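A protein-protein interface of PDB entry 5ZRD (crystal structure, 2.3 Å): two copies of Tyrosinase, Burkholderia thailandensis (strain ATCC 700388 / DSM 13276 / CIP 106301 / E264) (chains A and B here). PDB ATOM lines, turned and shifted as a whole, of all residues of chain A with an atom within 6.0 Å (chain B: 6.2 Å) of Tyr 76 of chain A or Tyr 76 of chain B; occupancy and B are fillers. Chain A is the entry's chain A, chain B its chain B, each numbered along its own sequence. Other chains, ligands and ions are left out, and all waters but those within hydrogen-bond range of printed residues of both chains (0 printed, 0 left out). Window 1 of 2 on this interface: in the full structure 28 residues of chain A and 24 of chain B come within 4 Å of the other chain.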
ATOM      1  N   ARG A  64     -19.732  -3.142   3.558  1.00  0.00           N
ATOM      2  CA  ARG A  64     -19.198  -1.924   4.132  1.00  0.00           C
ATOM      3  C   ARG A  64     -19.109  -2.150   5.649  1.00  0.00           C
ATOM      4  O   ARG A  64     -20.011  -1.757   6.459  1.00  0.00           O
ATOM      5  CB  ARG A  64     -20.083  -0.724   3.770  1.00  0.00           C
ATOM      6  CG  ARG A  64     -20.166  -0.412   2.275  1.00  0.00           C
ATOM      7  CD  ARG A  64     -21.276   0.592   1.973  1.00  0.00           C
ATOM      8  NE  ARG A  64     -21.553   0.741   0.559  1.00  0.00           N
ATOM      9  CZ  ARG A  64     -21.335   1.839  -0.161  1.00  0.00           C
ATOM     10  NH1 ARG A  64     -20.735   2.874   0.400  1.00  0.00           N
ATOM     11  NH2 ARG A  64     -21.703   1.884  -1.440  1.00  0.00           N
ATOM     12  N   VAL A  67     -19.706   0.575   8.030  1.00  0.00           N
ATOM     13  CA  VAL A  67     -21.154   0.895   8.146  1.00  0.00           C
ATOM     14  C   VAL A  67     -21.861  -0.177   8.990  1.00  0.00           C
ATOM     15  O   VAL A  67     -22.701   0.157   9.839  1.00  0.00           O
ATOM     16  CB  VAL A  67     -21.843   1.042   6.772  1.00  0.00           C
ATOM     17  CG1 VAL A  67     -23.332   1.227   6.899  1.00  0.00           C
ATOM     18  CG2 VAL A  67     -21.272   2.169   5.942  1.00  0.00           C
ATOM     19  N   LEU A  70     -21.769   0.539  12.641  1.00  0.00           N
ATOM     20  CA  LEU A  70     -22.278   1.813  13.217  1.00  0.00           C
ATOM     21  C   LEU A  70     -23.396   1.567  14.255  1.00  0.00           C
ATOM     22  O   LEU A  70     -24.174   0.624  14.134  1.00  0.00           O
ATOM     23  CB  LEU A  70     -22.810   2.695  12.083  1.00  0.00           C
ATOM     24  CG  LEU A  70     -21.764   3.240  11.122  1.00  0.00           C
ATOM     25  CD1 LEU A  70     -22.431   3.758   9.849  1.00  0.00           C
ATOM     26  CD2 LEU A  70     -20.934   4.322  11.806  1.00  0.00           C
ATOM     27  N   ASP A  73     -28.374   5.028  15.662  1.00  0.00           N
ATOM     28  CA  ASP A  73     -28.637   6.369  15.181  1.00  0.00           C
ATOM     29  C   ASP A  73     -27.754   6.866  14.061  1.00  0.00           C
ATOM     30  O   ASP A  73     -27.907   7.986  13.643  1.00  0.00           O
ATOM     31  CB  ASP A  73     -28.513   7.355  16.334  1.00  0.00           C
ATOM     32  CG  ASP A  73     -29.622   7.189  17.334  1.00  0.00           C
ATOM     33  OD1 ASP A  73     -30.706   6.688  16.947  1.00  0.00           O
ATOM     34  OD2 ASP A  73     -29.414   7.551  18.509  1.00  0.00           O
ATOM     35  N   ASP A  74     -26.817   6.052  13.600  1.00  0.00           N
ATOM     36  CA  ASP A  74     -25.825   6.501  12.644  1.00  0.00           C
ATOM     37  C   ASP A  74     -25.850   5.664  11.390  1.00  0.00           C
ATOM     38  O   ASP A  74     -25.315   6.074  10.337  1.00  0.00           O
ATOM     39  CB  ASP A  74     -24.422   6.381  13.265  1.00  0.00           C
ATOM     40  CG  ASP A  74     -24.120   7.445  14.325  1.00  0.00           C
ATOM     41  OD1 ASP A  74     -24.945   8.349  14.576  1.00  0.00           O
ATOM     42  OD2 ASP A  74     -23.039   7.336  14.961  1.00  0.00           O
ATOM     43  N   ILE A  75     -26.400   4.456  11.529  1.00  0.00           N
ATOM     44  CA  ILE A  75     -26.347   3.406  10.486  1.00  0.00           C
ATOM     45  C   ILE A  75     -27.433   3.721   9.442  1.00  0.00           C
ATOM     46  O   ILE A  75     -28.433   4.394   9.733  1.00  0.00           O
ATOM     47  CB  ILE A  75     -26.555   1.993  11.092  1.00  0.00           C
ATOM     48  CG1 ILE A  75     -26.210   0.882  10.101  1.00  0.00           C
ATOM     49  CG2 ILE A  75     -27.976   1.828  11.628  1.00  0.00           C
ATOM     50  CD1 ILE A  75     -26.085  -0.518  10.729  1.00  0.00           C
ATOM     51  N   TYR A  76     -27.219   3.197   8.252  1.00  0.00           N
ATOM     52  CA  TYR A  76     -28.043   3.441   7.128  1.00  0.00           C
ATOM     53  C   TYR A  76     -27.945   2.211   6.236  1.00  0.00           C
ATOM     54  O   TYR A  76     -26.914   1.550   6.220  1.00  0.00           O
ATOM     55  CB  TYR A  76     -27.606   4.713   6.389  1.00  0.00           C
ATOM     56  CG  TYR A  76     -26.221   4.650   5.795  1.00  0.00           C
ATOM     57  CD1 TYR A  76     -25.988   4.053   4.575  1.00  0.00           C
ATOM     58  CD2 TYR A  76     -25.140   5.240   6.426  1.00  0.00           C
ATOM     59  CE1 TYR A  76     -24.719   4.005   4.011  1.00  0.00           C
ATOM     60  CE2 TYR A  76     -23.859   5.203   5.877  1.00  0.00           C
ATOM     61  CZ  TYR A  76     -23.641   4.583   4.666  1.00  0.00           C
ATOM     62  OH  TYR A  76     -22.388   4.539   4.109  1.00  0.00           O
ATOM     63  N   PRO A  77     -29.039   1.892   5.548  1.00  0.00           N
ATOM     64  CA  PRO A  77     -29.109   0.711   4.707  1.00  0.00           C
ATOM     65  C   PRO A  77     -28.279   0.888   3.436  1.00  0.00           C
ATOM     66  O   PRO A  77     -28.167   1.988   2.965  1.00  0.00           O
ATOM     67  CB  PRO A  77     -30.592   0.584   4.343  1.00  0.00           C
ATOM     68  CG  PRO A  77     -31.128   1.999   4.490  1.00  0.00           C
ATOM     69  CD  PRO A  77     -30.319   2.607   5.617  1.00  0.00           C
ATOM     70  N   TYR A  78     -27.707  -0.191   2.921  1.00  0.00           N
ATOM     71  CA  TYR A  78     -26.957  -0.187   1.670  1.00  0.00           C
ATOM     72  C   TYR A  78     -27.132  -1.557   1.010  1.00  0.00           C
ATOM     73  O   TYR A  78     -27.631  -2.480   1.659  1.00  0.00           O
ATOM     74  CB  TYR A  78     -25.483   0.153   1.903  1.00  0.00           C
ATOM     75  CG  TYR A  78     -24.681  -0.926   2.590  1.00  0.00           C
ATOM     76  CD1 TYR A  78     -24.678  -1.043   3.971  1.00  0.00           C
ATOM     77  CD2 TYR A  78     -23.901  -1.809   1.866  1.00  0.00           C
ATOM     78  CE1 TYR A  78     -23.916  -2.007   4.615  1.00  0.00           C
ATOM     79  CE2 TYR A  78     -23.150  -2.792   2.492  1.00  0.00           C
ATOM     80  CZ  TYR A  78     -23.153  -2.893   3.873  1.00  0.00           C
ATOM     81  OH  TYR A  78     -22.427  -3.875   4.491  1.00  0.00           O
ATOM     82  N   PRO A 357     -26.958   2.546  -1.174  1.00  0.00           N
ATOM     83  CA  PRO A 357     -25.957   2.575  -2.204  1.00  0.00           C
ATOM     84  C   PRO A 357     -25.376   1.199  -2.546  1.00  0.00           C
ATOM     85  O   PRO A 357     -25.152   0.337  -1.691  1.00  0.00           O
ATOM     86  CB  PRO A 357     -24.878   3.515  -1.666  1.00  0.00           C
ATOM     87  CG  PRO A 357     -25.160   3.628  -0.184  1.00  0.00           C
ATOM     88  CD  PRO A 357     -26.650   3.435  -0.042  1.00  0.00           C
ATOM     89  N   PRO A 363     -23.296   7.547   0.091  1.00  0.00           N
ATOM     90  CA  PRO A 363     -24.527   8.175   0.538  1.00  0.00           C
ATOM     91  C   PRO A 363     -24.686   9.563  -0.087  1.00  0.00           C
ATOM     92  O   PRO A 363     -23.724  10.276  -0.265  1.00  0.00           O
ATOM     93  CB  PRO A 363     -24.401   8.297   2.068  1.00  0.00           C
ATOM     94  CG  PRO A 363     -23.420   7.217   2.438  1.00  0.00           C
ATOM     95  CD  PRO A 363     -22.487   7.141   1.256  1.00  0.00           C
ATOM     96  N   THR A 480     -33.470  -1.461   9.958  1.00  0.00           N
ATOM     97  CA  THR A 480     -33.450  -0.409   8.898  1.00  0.00           C
ATOM     98  C   THR A 480     -34.803   0.324   8.910  1.00  0.00           C
ATOM     99  O   THR A 480     -35.791  -0.225   8.429  1.00  0.00           O
ATOM    100  CB  THR A 480     -33.095  -1.010   7.526  1.00  0.00           C
ATOM    101  OG1 THR A 480     -31.671  -1.017   7.417  1.00  0.00           O
ATOM    102  CG2 THR A 480     -33.665  -0.259   6.339  1.00  0.00           C
ATOM    103  N   ARG B  64     -20.705  12.687  16.116  1.00  0.00           N
ATOM    104  CA  ARG B  64     -20.907  11.269  15.939  1.00  0.00           C
ATOM    105  C   ARG B  64     -19.556  10.674  15.531  1.00  0.00           C
ATOM    106  O   ARG B  64     -19.215  10.622  14.330  1.00  0.00           O
ATOM    107  CB  ARG B  64     -21.972  10.986  14.861  1.00  0.00           C
ATOM    108  CG  ARG B  64     -23.289  11.740  14.993  1.00  0.00           C
ATOM    109  CD  ARG B  64     -24.160  11.601  13.733  1.00  0.00           C
ATOM    110  NE  ARG B  64     -25.420  12.349  13.798  1.00  0.00           N
ATOM    111  CZ  ARG B  64     -26.626  11.824  13.980  1.00  0.00           C
ATOM    112  NH1 ARG B  64     -26.798  10.512  13.853  1.00  0.00           N
ATOM    113  NH2 ARG B  64     -27.652  12.616  14.267  1.00  0.00           N
ATOM    114  N   VAL B  67     -19.236   8.011  12.754  1.00  0.00           N
ATOM    115  CA  VAL B  67     -19.476   8.576  11.396  1.00  0.00           C
ATOM    116  C   VAL B  67     -18.229   9.349  10.948  1.00  0.00           C
ATOM    117  O   VAL B  67     -17.827   9.241   9.778  1.00  0.00           O
ATOM    118  CB  VAL B  67     -20.728   9.473  11.378  1.00  0.00           C
ATOM    119  CG1 VAL B  67     -20.930  10.124  10.024  1.00  0.00           C
ATOM    120  CG2 VAL B  67     -21.978   8.712  11.817  1.00  0.00           C
ATOM    121  N   LEU B  70     -15.648   7.162   9.273  1.00  0.00           N
ATOM    122  CA  LEU B  70     -15.957   6.313   8.075  1.00  0.00           C
ATOM    123  C   LEU B  70     -15.055   6.692   6.903  1.00  0.00           C
ATOM    124  O   LEU B  70     -14.680   7.844   6.778  1.00  0.00           O
ATOM    125  CB  LEU B  70     -17.420   6.479   7.647  1.00  0.00           C
ATOM    126  CG  LEU B  70     -18.470   5.956   8.634  1.00  0.00           C
ATOM    127  CD1 LEU B  70     -19.848   6.515   8.304  1.00  0.00           C
ATOM    128  CD2 LEU B  70     -18.488   4.430   8.659  1.00  0.00           C
ATOM    129  N   ASP B  73     -16.032   6.527   0.857  1.00  0.00           N
ATOM    130  CA  ASP B  73     -17.314   6.080   0.266  1.00  0.00           C
ATOM    131  C   ASP B  73     -18.483   5.830   1.235  1.00  0.00           C
ATOM    132  O   ASP B  73     -19.562   5.611   0.801  1.00  0.00           O
ATOM    133  CB  ASP B  73     -17.086   4.772  -0.553  1.00  0.00           C
ATOM    134  CG  ASP B  73     -16.264   4.996  -1.843  1.00  0.00           C
ATOM    135  OD1 ASP B  73     -15.770   6.116  -2.072  1.00  0.00           O
ATOM    136  OD2 ASP B  73     -16.120   4.043  -2.653  1.00  0.00           O
ATOM    137  N   ASP B  74     -18.265   5.796   2.535  1.00  0.00           N
ATOM    138  CA  ASP B  74     -19.297   5.416   3.481  1.00  0.00           C
ATOM    139  C   ASP B  74     -19.795   6.623   4.234  1.00  0.00           C
ATOM    140  O   ASP B  74     -20.803   6.560   4.937  1.00  0.00           O
ATOM    141  CB  ASP B  74     -18.743   4.379   4.486  1.00  0.00           C
ATOM    142  CG  ASP B  74     -18.298   3.065   3.817  1.00  0.00           C
ATOM    143  OD1 ASP B  74     -18.720   2.781   2.660  1.00  0.00           O
ATOM    144  OD2 ASP B  74     -17.503   2.305   4.438  1.00  0.00           O
ATOM    145  N   ILE B  75     -19.083   7.746   4.110  1.00  0.00           N
ATOM    146  CA  ILE B  75     -19.270   8.842   5.073  1.00  0.00           C
ATOM    147  C   ILE B  75     -20.447   9.677   4.574  1.00  0.00           C
ATOM    148  O   ILE B  75     -20.704   9.699   3.389  1.00  0.00           O
ATOM    149  CB  ILE B  75     -17.992   9.693   5.291  1.00  0.00           C
ATOM    150  CG1 ILE B  75     -18.141  10.590   6.526  1.00  0.00           C
ATOM    151  CG2 ILE B  75     -17.625  10.518   4.054  1.00  0.00           C
ATOM    152  CD1 ILE B  75     -16.854  11.264   6.990  1.00  0.00           C
ATOM    153  N   TYR B  76     -21.133  10.344   5.491  1.00  0.00           N
ATOM    154  CA  TYR B  76     -22.180  11.287   5.120  1.00  0.00           C
ATOM    155  C   TYR B  76     -22.108  12.539   6.000  1.00  0.00           C
ATOM    156  O   TYR B  76     -21.647  12.487   7.137  1.00  0.00           O
ATOM    157  CB  TYR B  76     -23.564  10.629   5.224  1.00  0.00           C
ATOM    158  CG  TYR B  76     -23.907  10.073   6.581  1.00  0.00           C
ATOM    159  CD1 TYR B  76     -24.473  10.879   7.547  1.00  0.00           C
ATOM    160  CD2 TYR B  76     -23.676   8.742   6.905  1.00  0.00           C
ATOM    161  CE1 TYR B  76     -24.861  10.378   8.774  1.00  0.00           C
ATOM    162  CE2 TYR B  76     -24.037   8.226   8.145  1.00  0.00           C
ATOM    163  CZ  TYR B  76     -24.622   9.047   9.088  1.00  0.00           C
ATOM    164  OH  TYR B  76     -24.995   8.594  10.326  1.00  0.00           O
ATOM    165  N   PRO B  77     -22.664  13.641   5.495  1.00  0.00           N
ATOM    166  CA  PRO B  77     -22.807  14.864   6.305  1.00  0.00           C
ATOM    167  C   PRO B  77     -23.852  14.791   7.429  1.00  0.00           C
ATOM    168  O   PRO B  77     -24.937  14.217   7.289  1.00  0.00           O
ATOM    169  CB  PRO B  77     -23.220  15.978   5.315  1.00  0.00           C
ATOM    170  CG  PRO B  77     -23.755  15.243   4.096  1.00  0.00           C
ATOM    171  CD  PRO B  77     -23.136  13.859   4.111  1.00  0.00           C
ATOM    172  N   TYR B  78     -23.549  15.449   8.516  1.00  0.00           N
ATOM    173  CA  TYR B  78     -24.519  15.655   9.562  1.00  0.00           C
ATOM    174  C   TYR B  78     -24.167  16.979  10.230  1.00  0.00           C
ATOM    175  O   TYR B  78     -23.097  17.518   9.953  1.00  0.00           O
ATOM    176  CB  TYR B  78     -24.490  14.507  10.573  1.00  0.00           C
ATOM    177  CG  TYR B  78     -23.238  14.444  11.416  1.00  0.00           C
ATOM    178  CD1 TYR B  78     -22.034  13.974  10.903  1.00  0.00           C
ATOM    179  CD2 TYR B  78     -23.241  14.899  12.723  1.00  0.00           C
ATOM    180  CE1 TYR B  78     -20.887  13.903  11.679  1.00  0.00           C
ATOM    181  CE2 TYR B  78     -22.109  14.820  13.519  1.00  0.00           C
ATOM    182  CZ  TYR B  78     -20.922  14.334  12.996  1.00  0.00           C
ATOM    183  OH  TYR B  78     -19.828  14.261  13.812  1.00  0.00           O
ATOM    184  N   PRO B 357     -28.239  15.017   9.448  1.00  0.00           N
ATOM    185  CA  PRO B 357     -29.051  14.924  10.658  1.00  0.00           C
ATOM    186  C   PRO B 357     -28.529  15.749  11.853  1.00  0.00           C
ATOM    187  O   PRO B 357     -27.343  15.948  11.989  1.00  0.00           O
ATOM    188  CB  PRO B 357     -29.074  13.433  11.025  1.00  0.00           C
ATOM    189  CG  PRO B 357     -28.393  12.703   9.888  1.00  0.00           C
ATOM    190  CD  PRO B 357     -27.992  13.725   8.842  1.00  0.00           C
ATOM    191  N   ALA B 362     -31.636  10.139  12.968  1.00  0.00           N
ATOM    192  CA  ALA B 362     -30.998   9.058  12.244  1.00  0.00           C
ATOM    193  C   ALA B 362     -31.017   9.406  10.760  1.00  0.00           C
ATOM    194  O   ALA B 362     -31.902  10.112  10.367  1.00  0.00           O
ATOM    195  CB  ALA B 362     -31.737   7.770  12.485  1.00  0.00           C
ATOM    196  N   PRO B 363     -30.044   8.923   9.973  1.00  0.00           N
ATOM    197  CA  PRO B 363     -30.138   9.025   8.524  1.00  0.00           C
ATOM    198  C   PRO B 363     -31.445   8.394   8.026  1.00  0.00           C
ATOM    199  O   PRO B 363     -31.827   7.322   8.500  1.00  0.00           O
ATOM    200  CB  PRO B 363     -28.948   8.257   7.916  1.00  0.00           C
ATOM    201  CG  PRO B 363     -28.022   8.008   9.071  1.00  0.00           C
ATOM    202  CD  PRO B 363     -28.848   8.171  10.338  1.00  0.00           C
ATOM    203  N   THR B 480     -17.859  16.990   2.402  1.00  0.00           N
ATOM    204  CA  THR B 480     -19.243  16.646   1.972  1.00  0.00           C
ATOM    205  C   THR B 480     -19.348  16.793   0.440  1.00  0.00           C
ATOM    206  O   THR B 480     -19.490  17.926  -0.069  1.00  0.00           O
ATOM    207  CB  THR B 480     -20.314  17.475   2.709  1.00  0.00           C
ATOM    208  OG1 THR B 480     -20.473  18.739   2.058  1.00  0.00           O
ATOM    209  CG2 THR B 480     -20.021  17.699   4.181  1.00  0.00           C
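Of the 13 printed residues of chain B, 9 touch a printed residue of chain A. Printed residues of chain B that touch a printed residue of chain A: Arg 64, Val 67, Leu 70, Asp 73, Asp 74, Ile 75, Tyr 76, Ala 362 and Pro 363. Among the printed residues, 17 pairs touch across the chains. Among the printed residues, Asp or Glu carboxylates within 4 Å of a Lys or Arg side-chain nitrogen of the other chain: Arg 64 of chain A with Asp 74 of chain B (3.0 Å) and Asp 74 of chain A with Arg 64 of chain B (2.9 Å).
Printed residues of chain B within 4 Å of Arg 64 of chain A: Asp 73 and Asp 74. Of the printed residues of chain B, Val 67 of chain A touches Asp 74. Of chain B, only Asp 74 (2.7 Å) and Tyr 76 (3.6 Å) come within 4 Å of Tyr 76 of chain A. Of the printed residues of chain A, Arg 64 of chain B touches Asp 73 and Asp 74. Of the printed residues of chain A, Tyr 76 of chain B touches Asp 74 and Tyr 76. The nearest residue of chain B that does not touch Tyr 76 of chain A is Pro 363 of chain B (4.1 Å). The nearest printed residue of chain A that does not touch Tyr 76 of chain B is Pro 363 of chain A (4.01 Å).
The backbone NH of Arg 64 of chain A is in hydrogen-bond range of the side-chain hydroxyl of Tyr 78 of chain A, 2.9 Å away. N of Arg 64 of chain B is in hydrogen-bond range of OH of Tyr 78 of chain B (2.9 Å).
Asp 74 of chain B touches Val 67 of chain A. Leu 70 of chain A touches Leu 70 of chain B. Ala 362 of chain B touches Asp 73 of chain A (CA to O, 3.6 Å). Val 67 of chain B touches Asp 74 of chain A. Pro 363 of chain B touches Asp 74 of chain A (CG to O, 3.6 Å). Ile 75 of chain A touches Pro 363 of chain B (O to CG, 3.7 Å). Tyr 76 of chain B touches Tyr 76 of chain A (CE2 to CD2, 3.6 Å). Asp 73 of chain B touches Pro 363 of chain A. CG of Pro 363 of chain A touches O of Asp 74 of chain B, 3.7 Å away. O of Ile 75 of chain B touches CD of Pro 363 of chain A, at 3.8 Å.
O of Asp 73 of chain B is in hydrogen-bond range of NH1 of Arg 64 of chain A. The side-chain carboxylate (OD1) of Asp 74 of chain B is in salt-bridge range of the guanidinium group (NH1) of Arg 64 of chain A (3.0 Å). The backbone carbonyl oxygen (O) of Asp 73 of chain A sits at hydrogen-bond distance from the guanidinium group (NH1) of Arg 64 of chain B (2.8 Å). The side-chain carboxylate (OD1) of Asp 74 of chain A is in salt-bridge range of the guanidinium group (NH1) of Arg 64 of chain B (2.9 Å). The side-chain hydroxyl (OH) of Tyr 76 of chain B is in hydrogen-bond range of the backbone carbonyl oxygen (O) of Asp 74 of chain A, at 2.5 Å. The side-chain hydroxyl (OH) of Tyr 76 of chain A lies within hydrogen-bond range of the backbone carbonyl oxygen (O) of Asp 74 of chain B, 2.7 Å away.
Val 67 of chain A touches Asp 74 of chain B, and with the chains exchanged Asp 74 of chain A touches Val 67 of chain B. Asp 73 of chain A touches Pro 363 of chain B, and with the chains exchanged Pro 363 of chain A touches Asp 73 of chain B. Asp 74 of chain A touches Pro 363 of chain B, and with the chains exchanged Pro 363 of chain A touches Asp 74 of chain B. Ile 75 of chain A touches Pro 363 of chain B, and with the chains exchanged Pro 363 of chain A touches Ile 75 of chain B. Positions printed for both chains: 64, 67, 70, 73, 74, 75, 76, 77, 78, 357, 363 and 480. Of the 17 pairs that touch across the chains among the printed residues, 16 have their exchanged pair printed and touching as well.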
